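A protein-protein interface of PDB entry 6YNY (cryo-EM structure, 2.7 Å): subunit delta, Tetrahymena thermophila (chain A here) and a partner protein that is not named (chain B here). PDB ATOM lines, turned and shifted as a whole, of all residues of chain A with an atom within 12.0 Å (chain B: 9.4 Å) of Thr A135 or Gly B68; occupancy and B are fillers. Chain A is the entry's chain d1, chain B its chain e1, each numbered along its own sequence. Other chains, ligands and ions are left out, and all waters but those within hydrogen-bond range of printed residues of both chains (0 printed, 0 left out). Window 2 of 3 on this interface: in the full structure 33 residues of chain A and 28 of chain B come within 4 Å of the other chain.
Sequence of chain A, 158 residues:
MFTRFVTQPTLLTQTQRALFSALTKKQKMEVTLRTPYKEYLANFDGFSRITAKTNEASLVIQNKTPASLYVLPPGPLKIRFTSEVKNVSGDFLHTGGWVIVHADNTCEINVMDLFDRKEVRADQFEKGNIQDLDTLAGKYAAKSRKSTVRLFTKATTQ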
ATOM      1  N   ILE A 130      -6.788   4.740  10.329  1.00  0.00           N
ATOM      2  CA  ILE A 130      -8.224   4.687  10.579  1.00  0.00           C
ATOM      3  C   ILE A 130      -8.561   5.441  11.857  1.00  0.00           C
ATOM      4  O   ILE A 130      -9.623   6.067  11.957  1.00  0.00           O
ATOM      5  CB  ILE A 130      -8.706   3.224  10.643  1.00  0.00           C
ATOM      6  CG1 ILE A 130      -8.448   2.510   9.312  1.00  0.00           C
ATOM      7  CG2 ILE A 130     -10.186   3.164  10.994  1.00  0.00           C
ATOM      8  CD1 ILE A 130      -7.024   2.024   9.128  1.00  0.00           C
ATOM      9  N   GLN A 131      -7.674   5.394  12.847  1.00  0.00           N
ATOM     10  CA  GLN A 131      -7.921   6.063  14.116  1.00  0.00           C
ATOM     11  C   GLN A 131      -8.107   7.561  13.909  1.00  0.00           C
ATOM     12  O   GLN A 131      -7.413   8.187  13.103  1.00  0.00           O
ATOM     13  CB  GLN A 131      -6.763   5.808  15.079  1.00  0.00           C
ATOM     14  CG  GLN A 131      -5.419   6.315  14.578  1.00  0.00           C
ATOM     15  CD  GLN A 131      -4.295   6.057  15.563  1.00  0.00           C
ATOM     16  OE1 GLN A 131      -4.515   5.514  16.645  1.00  0.00           O
ATOM     17  NE2 GLN A 131      -3.081   6.445  15.189  1.00  0.00           N
ATOM     18  N   ASP A 132      -9.054   8.134  14.647  1.00  0.00           N
ATOM     19  CA  ASP A 132      -9.321   9.562  14.608  1.00  0.00           C
ATOM     20  C   ASP A 132      -9.685  10.030  16.009  1.00  0.00           C
ATOM     21  O   ASP A 132      -9.930   9.225  16.912  1.00  0.00           O
ATOM     22  CB  ASP A 132     -10.441   9.899  13.614  1.00  0.00           C
ATOM     23  CG  ASP A 132     -11.733   9.160  13.916  1.00  0.00           C
ATOM     24  OD1 ASP A 132     -11.739   8.315  14.836  1.00  0.00           O
ATOM     25  OD2 ASP A 132     -12.745   9.427  13.233  1.00  0.00           O
ATOM     26  N   LEU A 133      -9.718  11.346  16.184  1.00  0.00           N
ATOM     27  CA  LEU A 133     -10.019  11.956  17.472  1.00  0.00           C
ATOM     28  C   LEU A 133     -11.434  12.514  17.470  1.00  0.00           C
ATOM     29  O   LEU A 133     -11.860  13.157  16.506  1.00  0.00           O
ATOM     30  CB  LEU A 133      -9.020  13.069  17.792  1.00  0.00           C
ATOM     31  CG  LEU A 133      -7.547  12.649  17.781  1.00  0.00           C
ATOM     32  CD1 LEU A 133      -6.670  13.770  18.312  1.00  0.00           C
ATOM     33  CD2 LEU A 133      -7.334  11.376  18.584  1.00  0.00           C
ATOM     34  N   ASP A 134     -12.159  12.264  18.558  1.00  0.00           N
ATOM     35  CA  ASP A 134     -13.551  12.688  18.677  1.00  0.00           C
ATOM     36  C   ASP A 134     -13.575  14.153  19.094  1.00  0.00           C
ATOM     37  O   ASP A 134     -13.619  14.489  20.278  1.00  0.00           O
ATOM     38  CB  ASP A 134     -14.294  11.811  19.677  1.00  0.00           C
ATOM     39  CG  ASP A 134     -15.788  12.077  19.694  1.00  0.00           C
ATOM     40  OD1 ASP A 134     -16.199  13.218  19.395  1.00  0.00           O
ATOM     41  OD2 ASP A 134     -16.554  11.143  20.011  1.00  0.00           O
ATOM     42  N   THR A 135     -13.544  15.036  18.100  1.00  0.00           N
ATOM     43  CA  THR A 135     -13.658  16.468  18.322  1.00  0.00           C
ATOM     44  C   THR A 135     -14.595  17.039  17.267  1.00  0.00           C
ATOM     45  O   THR A 135     -15.053  16.333  16.364  1.00  0.00           O
ATOM     46  CB  THR A 135     -12.290  17.162  18.267  1.00  0.00           C
ATOM     47  OG1 THR A 135     -11.737  17.032  16.952  1.00  0.00           O
ATOM     48  CG2 THR A 135     -11.337  16.549  19.279  1.00  0.00           C
ATOM     49  N   LEU A 136     -14.879  18.337  17.382  1.00  0.00           N
ATOM     50  CA  LEU A 136     -15.721  18.988  16.386  1.00  0.00           C
ATOM     51  C   LEU A 136     -15.019  19.067  15.037  1.00  0.00           C
ATOM     52  O   LEU A 136     -15.677  19.006  13.992  1.00  0.00           O
ATOM     53  CB  LEU A 136     -16.113  20.383  16.866  1.00  0.00           C
ATOM     54  CG  LEU A 136     -16.921  21.225  15.876  1.00  0.00           C
ATOM     55  CD1 LEU A 136     -18.211  20.518  15.490  1.00  0.00           C
ATOM     56  CD2 LEU A 136     -17.210  22.595  16.463  1.00  0.00           C
ATOM     57  N   ALA A 137     -13.692  19.201  15.041  1.00  0.00           N
ATOM     58  CA  ALA A 137     -12.939  19.254  13.794  1.00  0.00           C
ATOM     59  C   ALA A 137     -12.663  17.859  13.249  1.00  0.00           C
ATOM     60  O   ALA A 137     -12.723  17.641  12.034  1.00  0.00           O
ATOM     61  CB  ALA A 137     -11.630  20.012  14.010  1.00  0.00           C
ATOM     62  N   GLY A 138     -12.358  16.904  14.129  1.00  0.00           N
ATOM     63  CA  GLY A 138     -12.127  15.543  13.676  1.00  0.00           C
ATOM     64  C   GLY A 138     -13.338  14.938  12.999  1.00  0.00           C
ATOM     65  O   GLY A 138     -13.204  14.045  12.157  1.00  0.00           O
ATOM     66  N   LYS A 139     -14.534  15.408  13.353  1.00  0.00           N
ATOM     67  CA  LYS A 139     -15.745  14.911  12.710  1.00  0.00           C
ATOM     68  C   LYS A 139     -15.749  15.254  11.225  1.00  0.00           C
ATOM     69  O   LYS A 139     -15.985  14.388  10.376  1.00  0.00           O
ATOM     70  CB  LYS A 139     -16.972  15.495  13.413  1.00  0.00           C
ATOM     71  CG  LYS A 139     -18.308  15.040  12.854  1.00  0.00           C
ATOM     72  CD  LYS A 139     -18.867  16.050  11.864  1.00  0.00           C
ATOM     73  CE  LYS A 139     -20.293  15.709  11.463  1.00  0.00           C
ATOM     74  NZ  LYS A 139     -20.405  14.366  10.831  1.00  0.00           N
ATOM     75  N   TYR A 140     -15.481  16.520  10.894  1.00  0.00           N
ATOM     76  CA  TYR A 140     -15.383  16.909   9.491  1.00  0.00           C
ATOM     77  C   TYR A 140     -14.155  16.301   8.828  1.00  0.00           C
ATOM     78  O   TYR A 140     -14.197  15.966   7.639  1.00  0.00           O
ATOM     79  CB  TYR A 140     -15.349  18.432   9.371  1.00  0.00           C
ATOM     80  CG  TYR A 140     -16.663  19.098   9.700  1.00  0.00           C
ATOM     81  CD1 TYR A 140     -17.629  19.289   8.723  1.00  0.00           C
ATOM     82  CD2 TYR A 140     -16.940  19.537  10.988  1.00  0.00           C
ATOM     83  CE1 TYR A 140     -18.832  19.896   9.016  1.00  0.00           C
ATOM     84  CE2 TYR A 140     -18.142  20.146  11.291  1.00  0.00           C
ATOM     85  CZ  TYR A 140     -19.084  20.323  10.300  1.00  0.00           C
ATOM     86  OH  TYR A 140     -20.283  20.927  10.595  1.00  0.00           O
ATOM     87  N   ALA A 141     -13.060  16.152   9.575  1.00  0.00           N
ATOM     88  CA  ALA A 141     -11.853  15.554   9.016  1.00  0.00           C
ATOM     89  C   ALA A 141     -12.137  14.161   8.472  1.00  0.00           C
ATOM     90  O   ALA A 141     -11.825  13.855   7.316  1.00  0.00           O
ATOM     91  CB  ALA A 141     -10.757  15.504  10.079  1.00  0.00           C
ATOM     92  N   ALA A 142     -12.736  13.301   9.298  1.00  0.00           N
ATOM     93  CA  ALA A 142     -13.103  11.969   8.832  1.00  0.00           C
ATOM     94  C   ALA A 142     -14.151  12.041   7.734  1.00  0.00           C
ATOM     95  O   ALA A 142     -14.143  11.217   6.812  1.00  0.00           O
ATOM     96  CB  ALA A 142     -13.617  11.129  10.000  1.00  0.00           C
ATOM     97  N   LYS A 143     -15.053  13.020   7.810  1.00  0.00           N
ATOM     98  CA  LYS A 143     -16.083  13.165   6.788  1.00  0.00           C
ATOM     99  C   LYS A 143     -15.463  13.274   5.402  1.00  0.00           C
ATOM    100  O   LYS A 143     -15.901  12.609   4.456  1.00  0.00           O
ATOM    101  CB  LYS A 143     -16.939  14.394   7.094  1.00  0.00           C
ATOM    102  CG  LYS A 143     -18.179  14.524   6.230  1.00  0.00           C
ATOM    103  CD  LYS A 143     -18.891  15.843   6.479  1.00  0.00           C
ATOM    104  CE  LYS A 143     -19.355  15.970   7.920  1.00  0.00           C
ATOM    105  NZ  LYS A 143     -20.227  17.158   8.118  1.00  0.00           N
ATOM    106  N   SER A 144     -14.435  14.112   5.261  1.00  0.00           N
ATOM    107  CA  SER A 144     -13.768  14.250   3.971  1.00  0.00           C
ATOM    108  C   SER A 144     -13.043  12.966   3.593  1.00  0.00           C
ATOM    109  O   SER A 144     -13.138  12.498   2.452  1.00  0.00           O
ATOM    110  CB  SER A 144     -12.792  15.423   4.013  1.00  0.00           C
ATOM    111  OG  SER A 144     -11.826  15.239   5.032  1.00  0.00           O
ATOM    112  N   ARG A 145     -12.310  12.380   4.542  1.00  0.00           N
ATOM    113  CA  ARG A 145     -11.565  11.160   4.253  1.00  0.00           C
ATOM    114  C   ARG A 145     -12.485  10.059   3.745  1.00  0.00           C
ATOM    115  O   ARG A 145     -12.153   9.355   2.784  1.00  0.00           O
ATOM    116  CB  ARG A 145     -10.824  10.697   5.506  1.00  0.00           C
ATOM    117  CG  ARG A 145     -10.138   9.354   5.356  1.00  0.00           C
ATOM    118  CD  ARG A 145      -9.058   9.164   6.403  1.00  0.00           C
ATOM    119  NE  ARG A 145      -9.555   9.439   7.749  1.00  0.00           N
ATOM    120  CZ  ARG A 145     -10.217   8.562   8.497  1.00  0.00           C
ATOM    121  NH1 ARG A 145     -10.626   8.906   9.711  1.00  0.00           N
ATOM    122  NH2 ARG A 145     -10.480   7.347   8.035  1.00  0.00           N
ATOM    123  N   LYS A 146     -13.650   9.900   4.374  1.00  0.00           N
ATOM    124  CA  LYS A 146     -14.606   8.897   3.918  1.00  0.00           C
ATOM    125  C   LYS A 146     -15.118   9.226   2.523  1.00  0.00           C
ATOM    126  O   LYS A 146     -15.300   8.329   1.691  1.00  0.00           O
ATOM    127  CB  LYS A 146     -15.765   8.803   4.905  1.00  0.00           C
ATOM    128  CG  LYS A 146     -15.359   8.320   6.287  1.00  0.00           C
ATOM    129  CD  LYS A 146     -16.549   8.229   7.227  1.00  0.00           C
ATOM    130  CE  LYS A 146     -17.161   9.597   7.497  1.00  0.00           C
ATOM    131  NZ  LYS A 146     -18.271   9.528   8.486  1.00  0.00           N
ATOM    132  N   ALA B   6     -16.634  22.210   6.846  1.00  0.00           N
ATOM    133  CA  ALA B   6     -15.455  21.869   7.632  1.00  0.00           C
ATOM    134  C   ALA B   6     -14.734  23.119   8.110  1.00  0.00           C
ATOM    135  O   ALA B   6     -14.148  23.121   9.197  1.00  0.00           O
ATOM    136  CB  ALA B   6     -14.513  20.992   6.809  1.00  0.00           C
ATOM    137  N   PHE B   7     -14.767  24.188   7.316  1.00  0.00           N
ATOM    138  CA  PHE B   7     -14.139  25.443   7.699  1.00  0.00           C
ATOM    139  C   PHE B   7     -15.087  26.359   8.455  1.00  0.00           C
ATOM    140  O   PHE B   7     -14.626  27.216   9.216  1.00  0.00           O
ATOM    141  CB  PHE B   7     -13.612  26.165   6.455  1.00  0.00           C
ATOM    142  CG  PHE B   7     -13.054  27.528   6.736  1.00  0.00           C
ATOM    143  CD1 PHE B   7     -11.794  27.674   7.287  1.00  0.00           C
ATOM    144  CD2 PHE B   7     -13.783  28.664   6.437  1.00  0.00           C
ATOM    145  CE1 PHE B   7     -11.275  28.927   7.541  1.00  0.00           C
ATOM    146  CE2 PHE B   7     -13.269  29.920   6.687  1.00  0.00           C
ATOM    147  CZ  PHE B   7     -12.015  30.051   7.241  1.00  0.00           C
ATOM    148  N   LYS B   8     -16.398  26.197   8.267  1.00  0.00           N
ATOM    149  CA  LYS B   8     -17.368  27.058   8.935  1.00  0.00           C
ATOM    150  C   LYS B   8     -17.528  26.656  10.396  1.00  0.00           C
ATOM    151  O   LYS B   8     -17.304  27.463  11.304  1.00  0.00           O
ATOM    152  CB  LYS B   8     -18.713  26.986   8.208  1.00  0.00           C
ATOM    153  CG  LYS B   8     -19.800  27.889   8.781  1.00  0.00           C
ATOM    154  CD  LYS B   8     -19.399  29.362   8.796  1.00  0.00           C
ATOM    155  CE  LYS B   8     -19.072  29.879   7.405  1.00  0.00           C
ATOM    156  NZ  LYS B   8     -18.778  31.338   7.406  1.00  0.00           N
ATOM    157  N   LYS B   9     -17.918  25.403  10.635  1.00  0.00           N
ATOM    158  CA  LYS B   9     -18.130  24.907  11.986  1.00  0.00           C
ATOM    159  C   LYS B   9     -16.832  24.527  12.683  1.00  0.00           C
ATOM    160  O   LYS B   9     -16.852  24.239  13.883  1.00  0.00           O
ATOM    161  CB  LYS B   9     -19.064  23.697  11.951  1.00  0.00           C
ATOM    162  CG  LYS B   9     -19.690  23.353  13.289  1.00  0.00           C
ATOM    163  CD  LYS B   9     -20.649  22.181  13.160  1.00  0.00           C
ATOM    164  CE  LYS B   9     -21.470  21.980  14.425  1.00  0.00           C
ATOM    165  NZ  LYS B   9     -22.311  23.167  14.748  1.00  0.00           N
ATOM    166  N   ALA B  10     -15.712  24.524  11.964  1.00  0.00           N
ATOM    167  CA  ALA B  10     -14.421  24.195  12.542  1.00  0.00           C
ATOM    168  C   ALA B  10     -13.344  24.975  11.805  1.00  0.00           C
ATOM    169  O   ALA B  10     -13.453  25.225  10.603  1.00  0.00           O
ATOM    170  CB  ALA B  10     -14.138  22.692  12.463  1.00  0.00           C
ATOM    171  N   GLY B  11     -12.305  25.357  12.538  1.00  0.00           N
ATOM    172  CA  GLY B  11     -11.214  26.107  11.950  1.00  0.00           C
ATOM    173  C   GLY B  11     -10.252  25.228  11.179  1.00  0.00           C
ATOM    174  O   GLY B  11      -9.049  25.226  11.454  1.00  0.00           O
ATOM    175  N   ILE B  12     -10.769  24.474  10.213  1.00  0.00           N
ATOM    176  CA  ILE B  12      -9.966  23.556   9.409  1.00  0.00           C
ATOM    177  C   ILE B  12      -9.629  24.259   8.097  1.00  0.00           C
ATOM    178  O   ILE B  12     -10.534  24.473   7.273  1.00  0.00           O
ATOM    179  CB  ILE B  12     -10.706  22.238   9.153  1.00  0.00           C
ATOM    180  CG1 ILE B  12     -11.140  21.609  10.476  1.00  0.00           C
ATOM    181  CG2 ILE B  12      -9.823  21.278   8.372  1.00  0.00           C
ATOM    182  CD1 ILE B  12     -11.893  20.308  10.319  1.00  0.00           C
ATOM    183  N   PRO B  13      -8.374  24.631   7.857  1.00  0.00           N
ATOM    184  CA  PRO B  13      -8.018  25.215   6.562  1.00  0.00           C
ATOM    185  C   PRO B  13      -8.157  24.203   5.437  1.00  0.00           C
ATOM    186  O   PRO B  13      -8.257  22.992   5.652  1.00  0.00           O
ATOM    187  CB  PRO B  13      -6.557  25.644   6.745  1.00  0.00           C
ATOM    188  CG  PRO B  13      -6.345  25.699   8.215  1.00  0.00           C
ATOM    189  CD  PRO B  13      -7.240  24.656   8.794  1.00  0.00           C
ATOM    190  N   ARG B  16      -5.237  21.574   5.280  1.00  0.00           N
ATOM    191  CA  ARG B  16      -5.421  20.512   6.262  1.00  0.00           C
ATOM    192  C   ARG B  16      -6.511  19.551   5.814  1.00  0.00           C
ATOM    193  O   ARG B  16      -6.417  18.340   6.045  1.00  0.00           O
ATOM    194  CB  ARG B  16      -5.757  21.109   7.629  1.00  0.00           C
ATOM    195  CG  ARG B  16      -6.161  20.074   8.666  1.00  0.00           C
ATOM    196  CD  ARG B  16      -6.324  20.690  10.041  1.00  0.00           C
ATOM    197  NE  ARG B  16      -6.746  19.707  11.033  1.00  0.00           N
ATOM    198  CZ  ARG B  16      -6.886  19.965  12.328  1.00  0.00           C
ATOM    199  NH1 ARG B  16      -6.638  21.178  12.802  1.00  0.00           N
ATOM    200  NH2 ARG B  16      -7.274  19.004  13.155  1.00  0.00           N
ATOM    201  N   HIS B  20      -6.107  15.529   5.517  1.00  0.00           N
ATOM    202  CA  HIS B  20      -6.996  14.532   6.102  1.00  0.00           C
ATOM    203  C   HIS B  20      -7.689  13.710   5.027  1.00  0.00           C
ATOM    204  O   HIS B  20      -7.968  12.523   5.235  1.00  0.00           O
ATOM    205  CB  HIS B  20      -8.029  15.213   6.998  1.00  0.00           C
ATOM    206  CG  HIS B  20      -7.482  15.660   8.315  1.00  0.00           C
ATOM    207  ND1 HIS B  20      -7.447  14.841   9.422  1.00  0.00           N
ATOM    208  CD2 HIS B  20      -6.950  16.842   8.705  1.00  0.00           C
ATOM    209  CE1 HIS B  20      -6.918  15.499  10.438  1.00  0.00           C
ATOM    210  NE2 HIS B  20      -6.607  16.715  10.030  1.00  0.00           N
ATOM    211  N   THR B  59      -1.642  16.907  11.044  1.00  0.00           N
ATOM    212  CA  THR B  59      -3.046  16.626  10.765  1.00  0.00           C
ATOM    213  C   THR B  59      -3.972  17.069  11.884  1.00  0.00           C
ATOM    214  O   THR B  59      -5.043  17.617  11.615  1.00  0.00           O
ATOM    215  CB  THR B  59      -3.248  15.128  10.514  1.00  0.00           C
ATOM    216  OG1 THR B  59      -2.780  14.383  11.645  1.00  0.00           O
ATOM    217  CG2 THR B  59      -2.492  14.692   9.270  1.00  0.00           C
ATOM    218  N   LEU B  60      -3.577  16.844  13.135  1.00  0.00           N
ATOM    219  CA  LEU B  60      -4.344  17.289  14.288  1.00  0.00           C
ATOM    220  C   LEU B  60      -4.004  18.744  14.580  1.00  0.00           C
ATOM    221  O   LEU B  60      -3.424  19.431  13.732  1.00  0.00           O
ATOM    222  CB  LEU B  60      -4.042  16.411  15.504  1.00  0.00           C
ATOM    223  CG  LEU B  60      -4.125  14.902  15.263  1.00  0.00           C
ATOM    224  CD1 LEU B  60      -3.764  14.141  16.529  1.00  0.00           C
ATOM    225  CD2 LEU B  60      -5.504  14.506  14.770  1.00  0.00           C
ATOM    226  N   GLN B  61      -4.351  19.224  15.771  1.00  0.00           N
ATOM    227  CA  GLN B  61      -4.021  20.591  16.150  1.00  0.00           C
ATOM    228  C   GLN B  61      -2.530  20.684  16.451  1.00  0.00           C
ATOM    229  O   GLN B  61      -2.129  20.998  17.577  1.00  0.00           O
ATOM    230  CB  GLN B  61      -4.858  21.034  17.352  1.00  0.00           C
ATOM    231  CG  GLN B  61      -4.579  22.458  17.819  1.00  0.00           C
ATOM    232  CD  GLN B  61      -5.721  23.047  18.625  1.00  0.00           C
ATOM    233  OE1 GLN B  61      -6.677  22.352  18.970  1.00  0.00           O
ATOM    234  NE2 GLN B  61      -5.628  24.337  18.927  1.00  0.00           N
ATOM    235  N   PHE B  64      -1.714  22.892  11.653  1.00  0.00           N
ATOM    236  CA  PHE B  64      -2.846  23.721  11.252  1.00  0.00           C
ATOM    237  C   PHE B  64      -3.897  23.621  12.351  1.00  0.00           C
ATOM    238  O   PHE B  64      -4.829  22.807  12.262  1.00  0.00           O
ATOM    239  CB  PHE B  64      -3.416  23.279   9.906  1.00  0.00           C
ATOM    240  CG  PHE B  64      -2.412  23.284   8.791  1.00  0.00           C
ATOM    241  CD1 PHE B  64      -2.138  24.447   8.093  1.00  0.00           C
ATOM    242  CD2 PHE B  64      -1.748  22.123   8.436  1.00  0.00           C
ATOM    243  CE1 PHE B  64      -1.217  24.453   7.065  1.00  0.00           C
ATOM    244  CE2 PHE B  64      -0.825  22.124   7.408  1.00  0.00           C
ATOM    245  CZ  PHE B  64      -0.560  23.290   6.723  1.00  0.00           C
ATOM    246  N   PRO B  65      -3.775  24.422  13.409  1.00  0.00           N
ATOM    247  CA  PRO B  65      -4.766  24.369  14.488  1.00  0.00           C
ATOM    248  C   PRO B  65      -6.178  24.579  13.964  1.00  0.00           C
ATOM    249  O   PRO B  65      -6.396  25.101  12.869  1.00  0.00           O
ATOM    250  CB  PRO B  65      -4.341  25.509  15.419  1.00  0.00           C
ATOM    251  CG  PRO B  65      -2.893  25.691  15.156  1.00  0.00           C
ATOM    252  CD  PRO B  65      -2.689  25.371  13.706  1.00  0.00           C
ATOM    253  N   SER B  66      -7.148  24.160  14.773  1.00  0.00           N
ATOM    254  CA  SER B  66      -8.548  24.293  14.406  1.00  0.00           C
ATOM    255  C   SER B  66      -9.370  24.548  15.659  1.00  0.00           C
ATOM    256  O   SER B  66      -8.999  24.134  16.760  1.00  0.00           O
ATOM    257  CB  SER B  66      -9.056  23.040  13.683  1.00  0.00           C
ATOM    258  OG  SER B  66     -10.436  23.148  13.384  1.00  0.00           O
ATOM    259  N   LYS B  67     -10.496  25.237  15.472  1.00  0.00           N
ATOM    260  CA  LYS B  67     -11.380  25.532  16.593  1.00  0.00           C
ATOM    261  C   LYS B  67     -11.958  24.255  17.188  1.00  0.00           C
ATOM    262  O   LYS B  67     -12.142  24.156  18.406  1.00  0.00           O
ATOM    263  CB  LYS B  67     -12.498  26.469  16.139  1.00  0.00           C
ATOM    264  CG  LYS B  67     -12.000  27.728  15.447  1.00  0.00           C
ATOM    265  CD  LYS B  67     -13.144  28.636  15.009  1.00  0.00           C
ATOM    266  CE  LYS B  67     -14.003  27.987  13.932  1.00  0.00           C
ATOM    267  NZ  LYS B  67     -15.007  28.933  13.370  1.00  0.00           N
ATOM    268  N   GLY B  68     -12.247  23.264  16.342  1.00  0.00           N
ATOM    269  CA  GLY B  68     -12.854  22.040  16.830  1.00  0.00           C
ATOM    270  C   GLY B  68     -11.959  21.254  17.765  1.00  0.00           C
ATOM    271  O   GLY B  68     -12.449  20.569  18.667  1.00  0.00           O
ATOM    272  N   ASP B  69     -10.648  21.336  17.569  1.00  0.00           N
ATOM    273  CA  ASP B  69      -9.704  20.629  18.426  1.00  0.00           C
ATOM    274  C   ASP B  69      -9.394  21.452  19.671  1.00  0.00           C
ATOM    275  O   ASP B  69     -10.302  21.906  20.367  1.00  0.00           O
ATOM    276  CB  ASP B  69      -8.417  20.315  17.662  1.00  0.00           C
ATOM    277  CG  ASP B  69      -8.618  19.266  16.586  1.00  0.00           C
ATOM    278  OD1 ASP B  69      -9.713  18.668  16.532  1.00  0.00           O
ATOM    279  OD2 ASP B  69      -7.680  19.039  15.793  1.00  0.00           O
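Hydrophobic or aromatic side chains of chain B within 4 Å of the printed part of chain A: Ala B6, Ala B10, Ile B12, His B20 and Leu B60.
Along chain B the printed residues that touch a printed residue of chain A span positions 6 to 69.
Among the printed residues, no Asp or Glu carboxylate lies within 4 Å of a Lys or Arg side-chain nitrogen of the other chain.
The side-chain hydroxyl (OG1) of Thr A135 lies within hydrogen-bond range of the side-chain carboxylate (OD1) of Asp B69 (2.6 Å).
The side-chain hydroxyl (OG1) of Thr A135 lies close to the backbone NH (N) of Ala A137, 3.5 Å away.
The backbone carbonyl oxygen (O) of Ala A141 is in hydrogen-bond range of the side-chain hydroxyl (OG) of Ser A144, at 2.7 Å.
NE of Arg B16 sits at hydrogen-bond distance from NE2 of His B20, at 3.2 Å.
NH2 of Arg B16 lies within salt-bridge range of OD2 of Asp B69.
NE2 of His B20 sits at hydrogen-bond distance from O of Thr B59 (2.4 Å).
The side-chain hydroxyl (OG) of Ser B66 sits close to the backbone NH (N) of Gly B68, at 3.5 Å.
Thr A135 touches two residues of chain B.
Printed residues of chain B within 4 Å of Leu A136: Lys B9 (3.1 Å) and Gly B68 (3.5 Å).
Printed residues of chain B within 4 Å of Ala A141: His B20.
Printed residues of chain B within 4 Å of Arg A145: His B20.
Of chain A, only Ala A137 comes within 4 Å of Ala B10.
No residue of chain A comes within 4 Å of Gly B11.
Of the printed residues of chain A, Ile B12 touches Ala A137 (3.3 Å).
No residue of chain A comes within 4 Å of Lys B67.
Gly B68 touches just these residues of chain A: Thr A135, Leu A136 and Ala A137.
The nearest residue of chain B that does not touch Thr A135 is Arg B16 (6.2 Å).
The nearest residue of chain A that does not touch Gly B68 is Gly A138 (5.7 Å).
Among the printed residues, merely in contact across the chains: Tyr A140 with Lys B9, Leu A136 with Lys B9, Ala A137 with Ile B12, Arg A145 with His B20, Ala A137 with Ser B66, Leu A133 with Leu B60, Thr A135 with Gly B68, Ala A141 with His B20, Ala A137 with Asp B69, Ala A137 with Gly B68, Leu A136 with Gly B68, Tyr A140 with Ala B6, Ala A137 with Ala B10 and Gly A138 with Asp B69.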
